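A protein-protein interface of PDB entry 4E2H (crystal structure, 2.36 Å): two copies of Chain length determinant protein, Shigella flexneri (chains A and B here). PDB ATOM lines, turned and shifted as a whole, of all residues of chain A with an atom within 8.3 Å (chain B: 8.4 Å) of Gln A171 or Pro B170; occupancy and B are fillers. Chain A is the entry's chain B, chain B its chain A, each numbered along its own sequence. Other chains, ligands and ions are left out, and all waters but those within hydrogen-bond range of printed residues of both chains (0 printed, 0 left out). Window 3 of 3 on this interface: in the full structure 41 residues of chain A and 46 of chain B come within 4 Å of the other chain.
The backbone NH (N) of Gln A171 is in hydrogen-bond range of the backbone carbonyl oxygen (O) of Leu A185, 3.0 Å away.
O of Lys A169 lies close to OE1 of Gln A171, at 3.1 Å.
Gln A171 touches just these residues of chain B: Pro B170 and Val B172.
Of chain A, only Gln A171 (3.96 Å), Phe A184 (3.98 Å) and Leu A185 (3.8 Å) come within 4 Å of Pro B170.
Printed residues of chain A within 4 Å of Gln B174: Gln A174.
Printed residues of chain B within 4 Å of Gln A173: Gln B173 (3.5 Å).
Of the printed residues of chain B, Ala A165 touches Ala B190 (3.99 Å).
Gly A187 touches none of the printed residues of chain B.
Leu B185 touches none of the printed residues of chain A.
The nearest printed residue of chain A that does not touch Val B178 is Leu A185 (5.1 Å).
Val A172 touches Gln B173, but with the chains exchanged Gln A173 does not touch Val B172 (5.3 Å).
Gln A174 touches Thr B175, but with the chains exchanged Thr A175 does not touch Gln B174 (5.2 Å).
Phe A184 touches Leu B186, but with the chains exchanged Leu A186 does not touch Phe B184 (14.7 Å).
Leu A185 touches Pro B170, but with the chains exchanged Pro A170 does not touch Leu B185 (12.1 Å).
Positions printed for both chains: 167, 168, 169, 170, 171, 172, 173, 174, 175, 183, 184, 185, 186, 187 and 188.
The backbone carbonyl oxygen (O) of Gln A171 sits close to the backbone carbonyl oxygen (O) of Val B172 (3.2 Å).
Hydrophobic or aromatic side chains of chain A that line the printed part of chain B: Ala A165, Val A172, Phe A184 and Leu A185.
Ala B190 touches Ala A165.
Val B172 touches Val A172.
CG2 of Thr B175 touches CG1 of Val A172 (3.8 Å).
Gln A173 touches Gln B173.
Gln A174 touches Thr B175 (O to N, 3.9 Å).
Pro B170 touches Phe A184 (CG to CE2, 3.98 Å).
Leu B186 touches Phe A184 (O to CZ, 3.6 Å).
CZ of Phe A184 touches CB of Ala B190, at 3.3 Å.
Pro B170 touches Leu A185 (CB to CD2, 3.8 Å).
CG2 of Thr B175 touches CD1 of Leu A185, at 3.95 Å.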
ATOM      1  N   TYR A 161     -22.518 -12.503 -19.142  1.00  0.00           N
ATOM      2  CA  TYR A 161     -22.111 -13.906 -19.215  1.00  0.00           C
ATOM      3  C   TYR A 161     -21.468 -14.309 -17.900  1.00  0.00           C
ATOM      4  O   TYR A 161     -21.783 -15.353 -17.342  1.00  0.00           O
ATOM      5  CB  TYR A 161     -21.115 -14.167 -20.362  1.00  0.00           C
ATOM      6  CG  TYR A 161     -21.476 -13.592 -21.724  1.00  0.00           C
ATOM      7  CD1 TYR A 161     -22.785 -13.270 -22.054  1.00  0.00           C
ATOM      8  CD2 TYR A 161     -20.489 -13.386 -22.687  1.00  0.00           C
ATOM      9  CE1 TYR A 161     -23.101 -12.752 -23.302  1.00  0.00           C
ATOM     10  CE2 TYR A 161     -20.788 -12.861 -23.934  1.00  0.00           C
ATOM     11  CZ  TYR A 161     -22.095 -12.545 -24.243  1.00  0.00           C
ATOM     12  OH  TYR A 161     -22.406 -12.029 -25.489  1.00  0.00           O
ATOM     13  N   ALA A 162     -20.543 -13.495 -17.401  1.00  0.00           N
ATOM     14  CA  ALA A 162     -19.850 -13.865 -16.170  1.00  0.00           C
ATOM     15  C   ALA A 162     -20.820 -13.896 -14.969  1.00  0.00           C
ATOM     16  O   ALA A 162     -20.833 -14.866 -14.230  1.00  0.00           O
ATOM     17  CB  ALA A 162     -18.677 -12.960 -15.900  1.00  0.00           C
ATOM     18  N   ALA A 165     -22.821 -17.049 -14.966  1.00  0.00           N
ATOM     19  CA  ALA A 165     -22.000 -18.220 -14.650  1.00  0.00           C
ATOM     20  C   ALA A 165     -21.326 -18.042 -13.294  1.00  0.00           C
ATOM     21  O   ALA A 165     -20.418 -18.813 -12.932  1.00  0.00           O
ATOM     22  CB  ALA A 165     -20.953 -18.441 -15.734  1.00  0.00           C
ATOM     23  N   GLN A 166     -21.770 -17.016 -12.566  1.00  0.00           N
ATOM     24  CA  GLN A 166     -21.208 -16.641 -11.272  1.00  0.00           C
ATOM     25  C   GLN A 166     -19.679 -16.715 -11.228  1.00  0.00           C
ATOM     26  O   GLN A 166     -19.130 -17.340 -10.326  1.00  0.00           O
ATOM     27  CB  GLN A 166     -21.792 -17.513 -10.162  1.00  0.00           C
ATOM     28  CG  GLN A 166     -23.317 -17.473 -10.063  1.00  0.00           C
ATOM     29  CD  GLN A 166     -23.862 -18.449  -9.030  1.00  0.00           C
ATOM     30  OE1 GLN A 166     -23.270 -19.507  -8.784  1.00  0.00           O
ATOM     31  NE2 GLN A 166     -24.990 -18.092  -8.410  1.00  0.00           N
ATOM     32  N   VAL A 167     -18.996 -16.088 -12.189  1.00  0.00           N
ATOM     33  CA  VAL A 167     -17.543 -15.954 -12.129  1.00  0.00           C
ATOM     34  C   VAL A 167     -17.177 -14.535 -11.687  1.00  0.00           C
ATOM     35  O   VAL A 167     -17.602 -13.548 -12.304  1.00  0.00           O
ATOM     36  CB  VAL A 167     -16.885 -16.224 -13.488  1.00  0.00           C
ATOM     37  CG1 VAL A 167     -15.367 -16.153 -13.356  1.00  0.00           C
ATOM     38  CG2 VAL A 167     -17.320 -17.563 -14.027  1.00  0.00           C
ATOM     39  N   THR A 168     -16.377 -14.426 -10.632  1.00  0.00           N
ATOM     40  CA  THR A 168     -16.035 -13.116 -10.098  1.00  0.00           C
ATOM     41  C   THR A 168     -14.532 -12.842 -10.231  1.00  0.00           C
ATOM     42  O   THR A 168     -14.087 -11.687 -10.247  1.00  0.00           O
ATOM     43  CB  THR A 168     -16.452 -13.009  -8.629  1.00  0.00           C
ATOM     44  OG1 THR A 168     -16.232 -14.276  -7.999  1.00  0.00           O
ATOM     45  CG2 THR A 168     -17.934 -12.639  -8.513  1.00  0.00           C
ATOM     46  N   LYS A 169     -13.762 -13.916 -10.341  1.00  0.00           N
ATOM     47  CA  LYS A 169     -12.318 -13.809 -10.388  1.00  0.00           C
ATOM     48  C   LYS A 169     -11.761 -14.533 -11.588  1.00  0.00           C
ATOM     49  O   LYS A 169     -12.334 -15.525 -12.049  1.00  0.00           O
ATOM     50  CB  LYS A 169     -11.696 -14.414  -9.128  1.00  0.00           C
ATOM     51  CG  LYS A 169     -12.190 -13.805  -7.824  1.00  0.00           C
ATOM     52  CD  LYS A 169     -11.718 -12.361  -7.658  1.00  0.00           C
ATOM     53  CE  LYS A 169     -11.256 -12.127  -6.220  1.00  0.00           C
ATOM     54  NZ  LYS A 169     -11.389 -10.698  -5.814  1.00  0.00           N
ATOM     55  N   PRO A 170     -10.618 -14.047 -12.082  1.00  0.00           N
ATOM     56  CA  PRO A 170      -9.944 -14.640 -13.239  1.00  0.00           C
ATOM     57  C   PRO A 170      -9.951 -16.167 -13.174  1.00  0.00           C
ATOM     58  O   PRO A 170      -9.655 -16.744 -12.126  1.00  0.00           O
ATOM     59  CB  PRO A 170      -8.512 -14.106 -13.117  1.00  0.00           C
ATOM     60  CG  PRO A 170      -8.675 -12.782 -12.437  1.00  0.00           C
ATOM     61  CD  PRO A 170      -9.851 -12.927 -11.500  1.00  0.00           C
ATOM     62  N   GLN A 171     -10.283 -16.794 -14.298  1.00  0.00           N
ATOM     63  CA  GLN A 171     -10.293 -18.245 -14.432  1.00  0.00           C
ATOM     64  C   GLN A 171      -9.044 -18.753 -15.168  1.00  0.00           C
ATOM     65  O   GLN A 171      -8.872 -19.968 -15.365  1.00  0.00           O
ATOM     66  CB  GLN A 171     -11.542 -18.683 -15.200  1.00  0.00           C
ATOM     67  CG  GLN A 171     -12.859 -18.264 -14.556  1.00  0.00           C
ATOM     68  CD  GLN A 171     -13.152 -19.037 -13.298  1.00  0.00           C
ATOM     69  OE1 GLN A 171     -13.441 -18.449 -12.253  1.00  0.00           O
ATOM     70  NE2 GLN A 171     -13.077 -20.368 -13.384  1.00  0.00           N
ATOM     71  N   VAL A 172      -8.173 -17.830 -15.578  1.00  0.00           N
ATOM     72  CA  VAL A 172      -7.019 -18.218 -16.392  1.00  0.00           C
ATOM     73  C   VAL A 172      -5.653 -17.866 -15.801  1.00  0.00           C
ATOM     74  O   VAL A 172      -5.409 -16.723 -15.375  1.00  0.00           O
ATOM     75  CB  VAL A 172      -7.135 -17.688 -17.854  1.00  0.00           C
ATOM     76  CG1 VAL A 172      -8.141 -18.511 -18.628  1.00  0.00           C
ATOM     77  CG2 VAL A 172      -7.544 -16.221 -17.865  1.00  0.00           C
ATOM     78  N   GLN A 173      -4.781 -18.875 -15.766  1.00  0.00           N
ATOM     79  CA  GLN A 173      -3.387 -18.689 -15.386  1.00  0.00           C
ATOM     80  C   GLN A 173      -2.642 -17.972 -16.521  1.00  0.00           C
ATOM     81  O   GLN A 173      -2.327 -16.782 -16.415  1.00  0.00           O
ATOM     82  CB  GLN A 173      -2.710 -20.034 -15.060  1.00  0.00           C
ATOM     83  CG  GLN A 173      -3.132 -20.678 -13.727  1.00  0.00           C
ATOM     84  CD  GLN A 173      -4.005 -21.924 -13.901  1.00  0.00           C
ATOM     85  OE1 GLN A 173      -3.533 -22.980 -14.329  1.00  0.00           O
ATOM     86  NE2 GLN A 173      -5.285 -21.798 -13.568  1.00  0.00           N
ATOM     87  N   GLN A 174      -2.374 -18.689 -17.610  1.00  0.00           N
ATOM     88  CA  GLN A 174      -1.703 -18.083 -18.756  1.00  0.00           C
ATOM     89  C   GLN A 174      -2.726 -17.374 -19.654  1.00  0.00           C
ATOM     90  O   GLN A 174      -3.753 -17.945 -20.038  1.00  0.00           O
ATOM     91  CB  GLN A 174      -0.838 -19.096 -19.513  1.00  0.00           C
ATOM     92  CG  GLN A 174       0.430 -19.503 -18.742  1.00  0.00           C
ATOM     93  CD  GLN A 174       0.212 -20.684 -17.792  1.00  0.00           C
ATOM     94  OE1 GLN A 174      -0.908 -21.190 -17.651  1.00  0.00           O
ATOM     95  NE2 GLN A 174       1.290 -21.130 -17.141  1.00  0.00           N
ATOM     96  N   THR A 175      -2.410 -16.128 -19.994  1.00  0.00           N
ATOM     97  CA  THR A 175      -3.409 -15.113 -20.301  1.00  0.00           C
ATOM     98  C   THR A 175      -3.059 -14.247 -21.512  1.00  0.00           C
ATOM     99  O   THR A 175      -2.609 -13.108 -21.340  1.00  0.00           O
ATOM    100  CB  THR A 175      -3.528 -14.173 -19.095  1.00  0.00           C
ATOM    101  N   THR A 182     -14.206 -15.430 -24.794  1.00  0.00           N
ATOM    102  CA  THR A 182     -13.315 -15.483 -23.638  1.00  0.00           C
ATOM    103  C   THR A 182     -13.247 -14.270 -22.675  1.00  0.00           C
ATOM    104  O   THR A 182     -12.687 -14.388 -21.583  1.00  0.00           O
ATOM    105  CB  THR A 182     -11.880 -15.777 -24.091  1.00  0.00           C
ATOM    106  OG1 THR A 182     -11.420 -14.691 -24.906  1.00  0.00           O
ATOM    107  CG2 THR A 182     -11.841 -17.072 -24.897  1.00  0.00           C
ATOM    108  N   LEU A 183     -13.792 -13.116 -23.029  1.00  0.00           N
ATOM    109  CA  LEU A 183     -13.712 -11.996 -22.075  1.00  0.00           C
ATOM    110  C   LEU A 183     -14.198 -12.342 -20.666  1.00  0.00           C
ATOM    111  O   LEU A 183     -13.541 -11.988 -19.677  1.00  0.00           O
ATOM    112  CB  LEU A 183     -14.448 -10.748 -22.578  1.00  0.00           C
ATOM    113  CG  LEU A 183     -13.578  -9.693 -23.263  1.00  0.00           C
ATOM    114  CD1 LEU A 183     -14.436  -8.771 -24.142  1.00  0.00           C
ATOM    115  CD2 LEU A 183     -12.772  -8.891 -22.230  1.00  0.00           C
ATOM    116  N   PHE A 184     -15.341 -13.022 -20.563  1.00  0.00           N
ATOM    117  CA  PHE A 184     -15.955 -13.265 -19.254  1.00  0.00           C
ATOM    118  C   PHE A 184     -15.023 -14.072 -18.331  1.00  0.00           C
ATOM    119  O   PHE A 184     -15.238 -14.150 -17.118  1.00  0.00           O
ATOM    120  CB  PHE A 184     -17.320 -13.967 -19.392  1.00  0.00           C
ATOM    121  CG  PHE A 184     -17.232 -15.477 -19.415  1.00  0.00           C
ATOM    122  CD1 PHE A 184     -16.954 -16.155 -20.591  1.00  0.00           C
ATOM    123  CD2 PHE A 184     -17.440 -16.218 -18.258  1.00  0.00           C
ATOM    124  CE1 PHE A 184     -16.871 -17.539 -20.613  1.00  0.00           C
ATOM    125  CE2 PHE A 184     -17.353 -17.603 -18.280  1.00  0.00           C
ATOM    126  CZ  PHE A 184     -17.066 -18.257 -19.458  1.00  0.00           C
ATOM    127  N   LEU A 185     -13.970 -14.658 -18.883  1.00  0.00           N
ATOM    128  CA  LEU A 185     -13.049 -15.376 -18.025  1.00  0.00           C
ATOM    129  C   LEU A 185     -12.310 -14.439 -17.079  1.00  0.00           C
ATOM    130  O   LEU A 185     -11.716 -14.893 -16.104  1.00  0.00           O
ATOM    131  CB  LEU A 185     -12.067 -16.182 -18.857  1.00  0.00           C
ATOM    132  CG  LEU A 185     -12.814 -17.160 -19.766  1.00  0.00           C
ATOM    133  CD1 LEU A 185     -11.907 -17.672 -20.891  1.00  0.00           C
ATOM    134  CD2 LEU A 185     -13.372 -18.302 -18.953  1.00  0.00           C
ATOM    135  N   LEU A 186     -12.329 -13.135 -17.349  1.00  0.00           N
ATOM    136  CA  LEU A 186     -11.620 -12.179 -16.469  1.00  0.00           C
ATOM    137  C   LEU A 186     -12.459 -12.005 -15.213  1.00  0.00           C
ATOM    138  O   LEU A 186     -12.026 -11.415 -14.214  1.00  0.00           O
ATOM    139  CB  LEU A 186     -11.413 -10.831 -17.150  1.00  0.00           C
ATOM    140  CG  LEU A 186     -10.815 -10.852 -18.561  1.00  0.00           C
ATOM    141  CD1 LEU A 186     -10.965  -9.502 -19.238  1.00  0.00           C
ATOM    142  CD2 LEU A 186      -9.361 -11.297 -18.549  1.00  0.00           C
ATOM    143  N   GLY A 187     -13.673 -12.541 -15.255  1.00  0.00           N
ATOM    144  CA  GLY A 187     -14.509 -12.487 -14.076  1.00  0.00           C
ATOM    145  C   GLY A 187     -15.096 -11.109 -13.898  1.00  0.00           C
ATOM    146  O   GLY A 187     -14.583 -10.119 -14.437  1.00  0.00           O
ATOM    147  N   SER A 188     -16.170 -11.060 -13.124  1.00  0.00           N
ATOM    148  CA  SER A 188     -17.066  -9.919 -13.092  1.00  0.00           C
ATOM    149  C   SER A 188     -16.506  -8.808 -12.231  1.00  0.00           C
ATOM    150  O   SER A 188     -16.878  -7.646 -12.388  1.00  0.00           O
ATOM    151  CB  SER A 188     -18.439 -10.350 -12.573  1.00  0.00           C
ATOM    152  OG  SER A 188     -18.280 -11.090 -11.378  1.00  0.00           O
ATOM    153  N   VAL B 167     -19.573 -30.017 -18.674  1.00  0.00           N
ATOM    154  CA  VAL B 167     -18.788 -28.824 -18.388  1.00  0.00           C
ATOM    155  C   VAL B 167     -19.832 -27.742 -18.180  1.00  0.00           C
ATOM    156  O   VAL B 167     -20.390 -27.200 -19.133  1.00  0.00           O
ATOM    157  CB  VAL B 167     -17.838 -28.418 -19.529  1.00  0.00           C
ATOM    158  CG1 VAL B 167     -16.715 -27.572 -18.956  1.00  0.00           C
ATOM    159  CG2 VAL B 167     -17.288 -29.644 -20.214  1.00  0.00           C
ATOM    160  N   THR B 168     -20.134 -27.452 -16.930  1.00  0.00           N
ATOM    161  CA  THR B 168     -21.228 -26.550 -16.660  1.00  0.00           C
ATOM    162  C   THR B 168     -20.623 -25.199 -16.320  1.00  0.00           C
ATOM    163  O   THR B 168     -21.243 -24.154 -16.505  1.00  0.00           O
ATOM    164  CB  THR B 168     -22.159 -27.108 -15.554  1.00  0.00           C
ATOM    165  OG1 THR B 168     -22.311 -26.147 -14.503  1.00  0.00           O
ATOM    166  CG2 THR B 168     -21.583 -28.409 -14.975  1.00  0.00           C
ATOM    167  N   LYS B 169     -19.384 -25.232 -15.850  1.00  0.00           N
ATOM    168  CA  LYS B 169     -18.654 -24.010 -15.585  1.00  0.00           C
ATOM    169  C   LYS B 169     -17.301 -24.068 -16.300  1.00  0.00           C
ATOM    170  O   LYS B 169     -16.761 -25.159 -16.535  1.00  0.00           O
ATOM    171  CB  LYS B 169     -18.547 -23.754 -14.066  1.00  0.00           C
ATOM    172  CG  LYS B 169     -19.931 -23.534 -13.407  1.00  0.00           C
ATOM    173  CD  LYS B 169     -19.850 -22.883 -12.022  1.00  0.00           C
ATOM    174  CE  LYS B 169     -19.609 -23.905 -10.898  1.00  0.00           C
ATOM    175  NZ  LYS B 169     -18.242 -23.780 -10.308  1.00  0.00           N
ATOM    176  N   PRO B 170     -16.768 -22.891 -16.672  1.00  0.00           N
ATOM    177  CA  PRO B 170     -15.570 -22.760 -17.503  1.00  0.00           C
ATOM    178  C   PRO B 170     -14.403 -23.568 -16.965  1.00  0.00           C
ATOM    179  O   PRO B 170     -13.966 -23.356 -15.834  1.00  0.00           O
ATOM    180  CB  PRO B 170     -15.258 -21.256 -17.446  1.00  0.00           C
ATOM    181  CG  PRO B 170     -16.012 -20.748 -16.243  1.00  0.00           C
ATOM    182  CD  PRO B 170     -17.255 -21.578 -16.225  1.00  0.00           C
ATOM    183  N   GLN B 171     -13.924 -24.513 -17.766  1.00  0.00           N
ATOM    184  CA  GLN B 171     -12.702 -25.216 -17.434  1.00  0.00           C
ATOM    185  C   GLN B 171     -11.677 -24.901 -18.516  1.00  0.00           C
ATOM    186  O   GLN B 171     -11.415 -25.735 -19.392  1.00  0.00           O
ATOM    187  CB  GLN B 171     -12.937 -26.735 -17.307  1.00  0.00           C
ATOM    188  CG  GLN B 171     -13.944 -27.195 -16.212  1.00  0.00           C
ATOM    189  CD  GLN B 171     -13.432 -27.087 -14.753  1.00  0.00           C
ATOM    190  OE1 GLN B 171     -13.781 -26.146 -14.028  1.00  0.00           O
ATOM    191  NE2 GLN B 171     -12.639 -28.077 -14.316  1.00  0.00           N
ATOM    192  N   VAL B 172     -11.127 -23.683 -18.456  1.00  0.00           N
ATOM    193  CA  VAL B 172     -10.026 -23.265 -19.322  1.00  0.00           C
ATOM    194  C   VAL B 172      -8.759 -23.061 -18.490  1.00  0.00           C
ATOM    195  O   VAL B 172      -8.762 -22.290 -17.521  1.00  0.00           O
ATOM    196  CB  VAL B 172     -10.327 -21.917 -20.017  1.00  0.00           C
ATOM    197  CG1 VAL B 172      -9.380 -21.684 -21.186  1.00  0.00           C
ATOM    198  CG2 VAL B 172     -11.760 -21.869 -20.481  1.00  0.00           C
ATOM    199  N   GLN B 173      -7.684 -23.753 -18.856  1.00  0.00           N
ATOM    200  CA  GLN B 173      -6.388 -23.465 -18.268  1.00  0.00           C
ATOM    201  C   GLN B 173      -5.836 -22.199 -18.926  1.00  0.00           C
ATOM    202  O   GLN B 173      -5.322 -21.314 -18.237  1.00  0.00           O
ATOM    203  CB  GLN B 173      -5.432 -24.645 -18.436  1.00  0.00           C
ATOM    204  N   GLN B 174      -5.958 -22.100 -20.253  1.00  0.00           N
ATOM    205  CA  GLN B 174      -5.551 -20.884 -20.969  1.00  0.00           C
ATOM    206  C   GLN B 174      -6.325 -20.613 -22.258  1.00  0.00           C
ATOM    207  O   GLN B 174      -6.748 -21.533 -22.975  1.00  0.00           O
ATOM    208  CB  GLN B 174      -4.065 -20.897 -21.284  1.00  0.00           C
ATOM    209  CG  GLN B 174      -3.659 -22.116 -22.050  1.00  0.00           C
ATOM    210  CD  GLN B 174      -2.185 -22.136 -22.428  1.00  0.00           C
ATOM    211  OE1 GLN B 174      -1.292 -22.176 -21.575  1.00  0.00           O
ATOM    212  NE2 GLN B 174      -1.927 -22.138 -23.725  1.00  0.00           N
ATOM    213  N   THR B 175      -6.447 -19.327 -22.570  1.00  0.00           N
ATOM    214  CA  THR B 175      -7.355 -18.862 -23.608  1.00  0.00           C
ATOM    215  C   THR B 175      -6.987 -19.220 -25.057  1.00  0.00           C
ATOM    216  O   THR B 175      -7.835 -19.139 -25.943  1.00  0.00           O
ATOM    217  CB  THR B 175      -7.617 -17.350 -23.473  1.00  0.00           C
ATOM    218  OG1 THR B 175      -6.392 -16.630 -23.660  1.00  0.00           O
ATOM    219  CG2 THR B 175      -8.190 -17.031 -22.078  1.00  0.00           C
ATOM    220  N   VAL B 178      -9.330 -22.016 -26.435  1.00  0.00           N
ATOM    221  CA  VAL B 178     -10.715 -21.733 -26.820  1.00  0.00           C
ATOM    222  C   VAL B 178     -10.787 -21.115 -28.223  1.00  0.00           C
ATOM    223  O   VAL B 178     -10.421 -19.954 -28.429  1.00  0.00           O
ATOM    224  CB  VAL B 178     -11.365 -20.741 -25.817  1.00  0.00           C
ATOM    225  CG1 VAL B 178     -12.716 -20.263 -26.297  1.00  0.00           C
ATOM    226  CG2 VAL B 178     -11.445 -21.337 -24.427  1.00  0.00           C
ATOM    227  N   LEU B 183     -15.430 -24.324 -28.324  1.00  0.00           N
ATOM    228  CA  LEU B 183     -16.150 -23.316 -27.584  1.00  0.00           C
ATOM    229  C   LEU B 183     -16.756 -23.842 -26.290  1.00  0.00           C
ATOM    230  O   LEU B 183     -16.959 -23.084 -25.339  1.00  0.00           O
ATOM    231  CB  LEU B 183     -17.207 -22.685 -28.482  1.00  0.00           C
ATOM    232  CG  LEU B 183     -16.592 -21.494 -29.214  1.00  0.00           C
ATOM    233  CD1 LEU B 183     -17.455 -21.065 -30.399  1.00  0.00           C
ATOM    234  CD2 LEU B 183     -16.425 -20.347 -28.225  1.00  0.00           C
ATOM    235  N   PHE B 184     -17.030 -25.139 -26.235  1.00  0.00           N
ATOM    236  CA  PHE B 184     -17.669 -25.728 -25.036  1.00  0.00           C
ATOM    237  C   PHE B 184     -16.762 -25.680 -23.802  1.00  0.00           C
ATOM    238  O   PHE B 184     -17.212 -25.926 -22.688  1.00  0.00           O
ATOM    239  CB  PHE B 184     -18.059 -27.176 -25.276  1.00  0.00           C
ATOM    240  CG  PHE B 184     -16.930 -28.012 -25.797  1.00  0.00           C
ATOM    241  CD1 PHE B 184     -15.969 -28.537 -24.934  1.00  0.00           C
ATOM    242  CD2 PHE B 184     -16.822 -28.268 -27.153  1.00  0.00           C
ATOM    243  CE1 PHE B 184     -14.926 -29.313 -25.434  1.00  0.00           C
ATOM    244  CE2 PHE B 184     -15.782 -29.031 -27.651  1.00  0.00           C
ATOM    245  CZ  PHE B 184     -14.835 -29.553 -26.795  1.00  0.00           C
ATOM    246  N   LEU B 185     -15.486 -25.357 -23.990  1.00  0.00           N
ATOM    247  CA  LEU B 185     -14.612 -25.196 -22.844  1.00  0.00           C
ATOM    248  C   LEU B 185     -15.179 -24.108 -21.952  1.00  0.00           C
ATOM    249  O   LEU B 185     -14.972 -24.138 -20.753  1.00  0.00           O
ATOM    250  CB  LEU B 185     -13.200 -24.838 -23.296  1.00  0.00           C
ATOM    251  CG  LEU B 185     -12.515 -25.931 -24.116  1.00  0.00           C
ATOM    252  CD1 LEU B 185     -11.178 -25.432 -24.607  1.00  0.00           C
ATOM    253  CD2 LEU B 185     -12.347 -27.218 -23.287  1.00  0.00           C
ATOM    254  N   LEU B 186     -15.902 -23.150 -22.535  1.00  0.00           N
ATOM    255  CA  LEU B 186     -16.437 -22.038 -21.748  1.00  0.00           C
ATOM    256  C   LEU B 186     -17.509 -22.462 -20.717  1.00  0.00           C
ATOM    257  O   LEU B 186     -17.840 -21.714 -19.783  1.00  0.00           O
ATOM    258  CB  LEU B 186     -16.977 -20.946 -22.668  1.00  0.00           C
ATOM    259  CG  LEU B 186     -16.029 -20.472 -23.786  1.00  0.00           C
ATOM    260  CD1 LEU B 186     -16.689 -19.379 -24.588  1.00  0.00           C
ATOM    261  CD2 LEU B 186     -14.706 -19.979 -23.235  1.00  0.00           C
ATOM    262  N   GLY B 187     -18.047 -23.666 -20.878  1.00  0.00           N
ATOM    263  CA  GLY B 187     -19.081 -24.127 -19.969  1.00  0.00           C
ATOM    264  C   GLY B 187     -20.496 -23.876 -20.461  1.00  0.00           C
ATOM    265  O   GLY B 187     -20.799 -22.811 -21.003  1.00  0.00           O
ATOM    266  N   SER B 188     -21.366 -24.861 -20.255  1.00  0.00           N
ATOM    267  CA  SER B 188     -22.776 -24.746 -20.606  1.00  0.00           C
ATOM    268  C   SER B 188     -23.487 -23.500 -20.056  1.00  0.00           C
ATOM    269  O   SER B 188     -24.453 -23.041 -20.667  1.00  0.00           O
ATOM    270  CB  SER B 188     -23.534 -25.987 -20.130  1.00  0.00           C
ATOM    271  OG  SER B 188     -23.663 -25.980 -18.714  1.00  0.00           O
ATOM    272  N   GLU B 189     -23.041 -22.970 -18.912  1.00  0.00           N
ATOM    273  CA  GLU B 189     -23.704 -21.806 -18.292  1.00  0.00           C
ATOM    274  C   GLU B 189     -23.481 -20.466 -19.025  1.00  0.00           C
ATOM    275  O   GLU B 189     -24.447 -19.808 -19.447  1.00  0.00           O
ATOM    276  CB  GLU B 189     -23.305 -21.664 -16.822  1.00  0.00           C
ATOM    277  CG  GLU B 189     -24.470 -21.775 -15.852  1.00  0.00           C
ATOM    278  CD  GLU B 189     -24.018 -22.284 -14.490  1.00  0.00           C
ATOM    279  OE1 GLU B 189     -22.780 -22.434 -14.313  1.00  0.00           O
ATOM    280  OE2 GLU B 189     -24.886 -22.539 -13.606  1.00  0.00           O
ATOM    281  N   ALA B 190     -22.212 -20.061 -19.155  1.00  0.00           N
ATOM    282  CA  ALA B 190     -21.837 -18.861 -19.914  1.00  0.00           C
ATOM    283  C   ALA B 190     -22.356 -19.062 -21.313  1.00  0.00           C
ATOM    284  O   ALA B 190     -22.834 -18.127 -21.949  1.00  0.00           O
ATOM    285  CB  ALA B 190     -20.292 -18.666 -19.950  1.00  0.00           C
ATOM    286  N   LEU B 191     -22.271 -20.302 -21.779  1.00  0.00           N
ATOM    287  CA  LEU B 191     -22.728 -20.642 -23.104  1.00  0.00           C
ATOM    288  C   LEU B 191     -24.223 -20.358 -23.242  1.00  0.00           C
ATOM    289  O   LEU B 191     -24.664 -19.834 -24.272  1.00  0.00           O
ATOM    290  CB  LEU B 191     -22.362 -22.089 -23.453  1.00  0.00           C
ATOM    291  CG  LEU B 191     -20.885 -22.243 -23.866  1.00  0.00           C
ATOM    292  CD1 LEU B 191     -20.466 -23.694 -24.178  1.00  0.00           C
ATOM    293  CD2 LEU B 191     -20.574 -21.321 -25.062  1.00  0.00           C
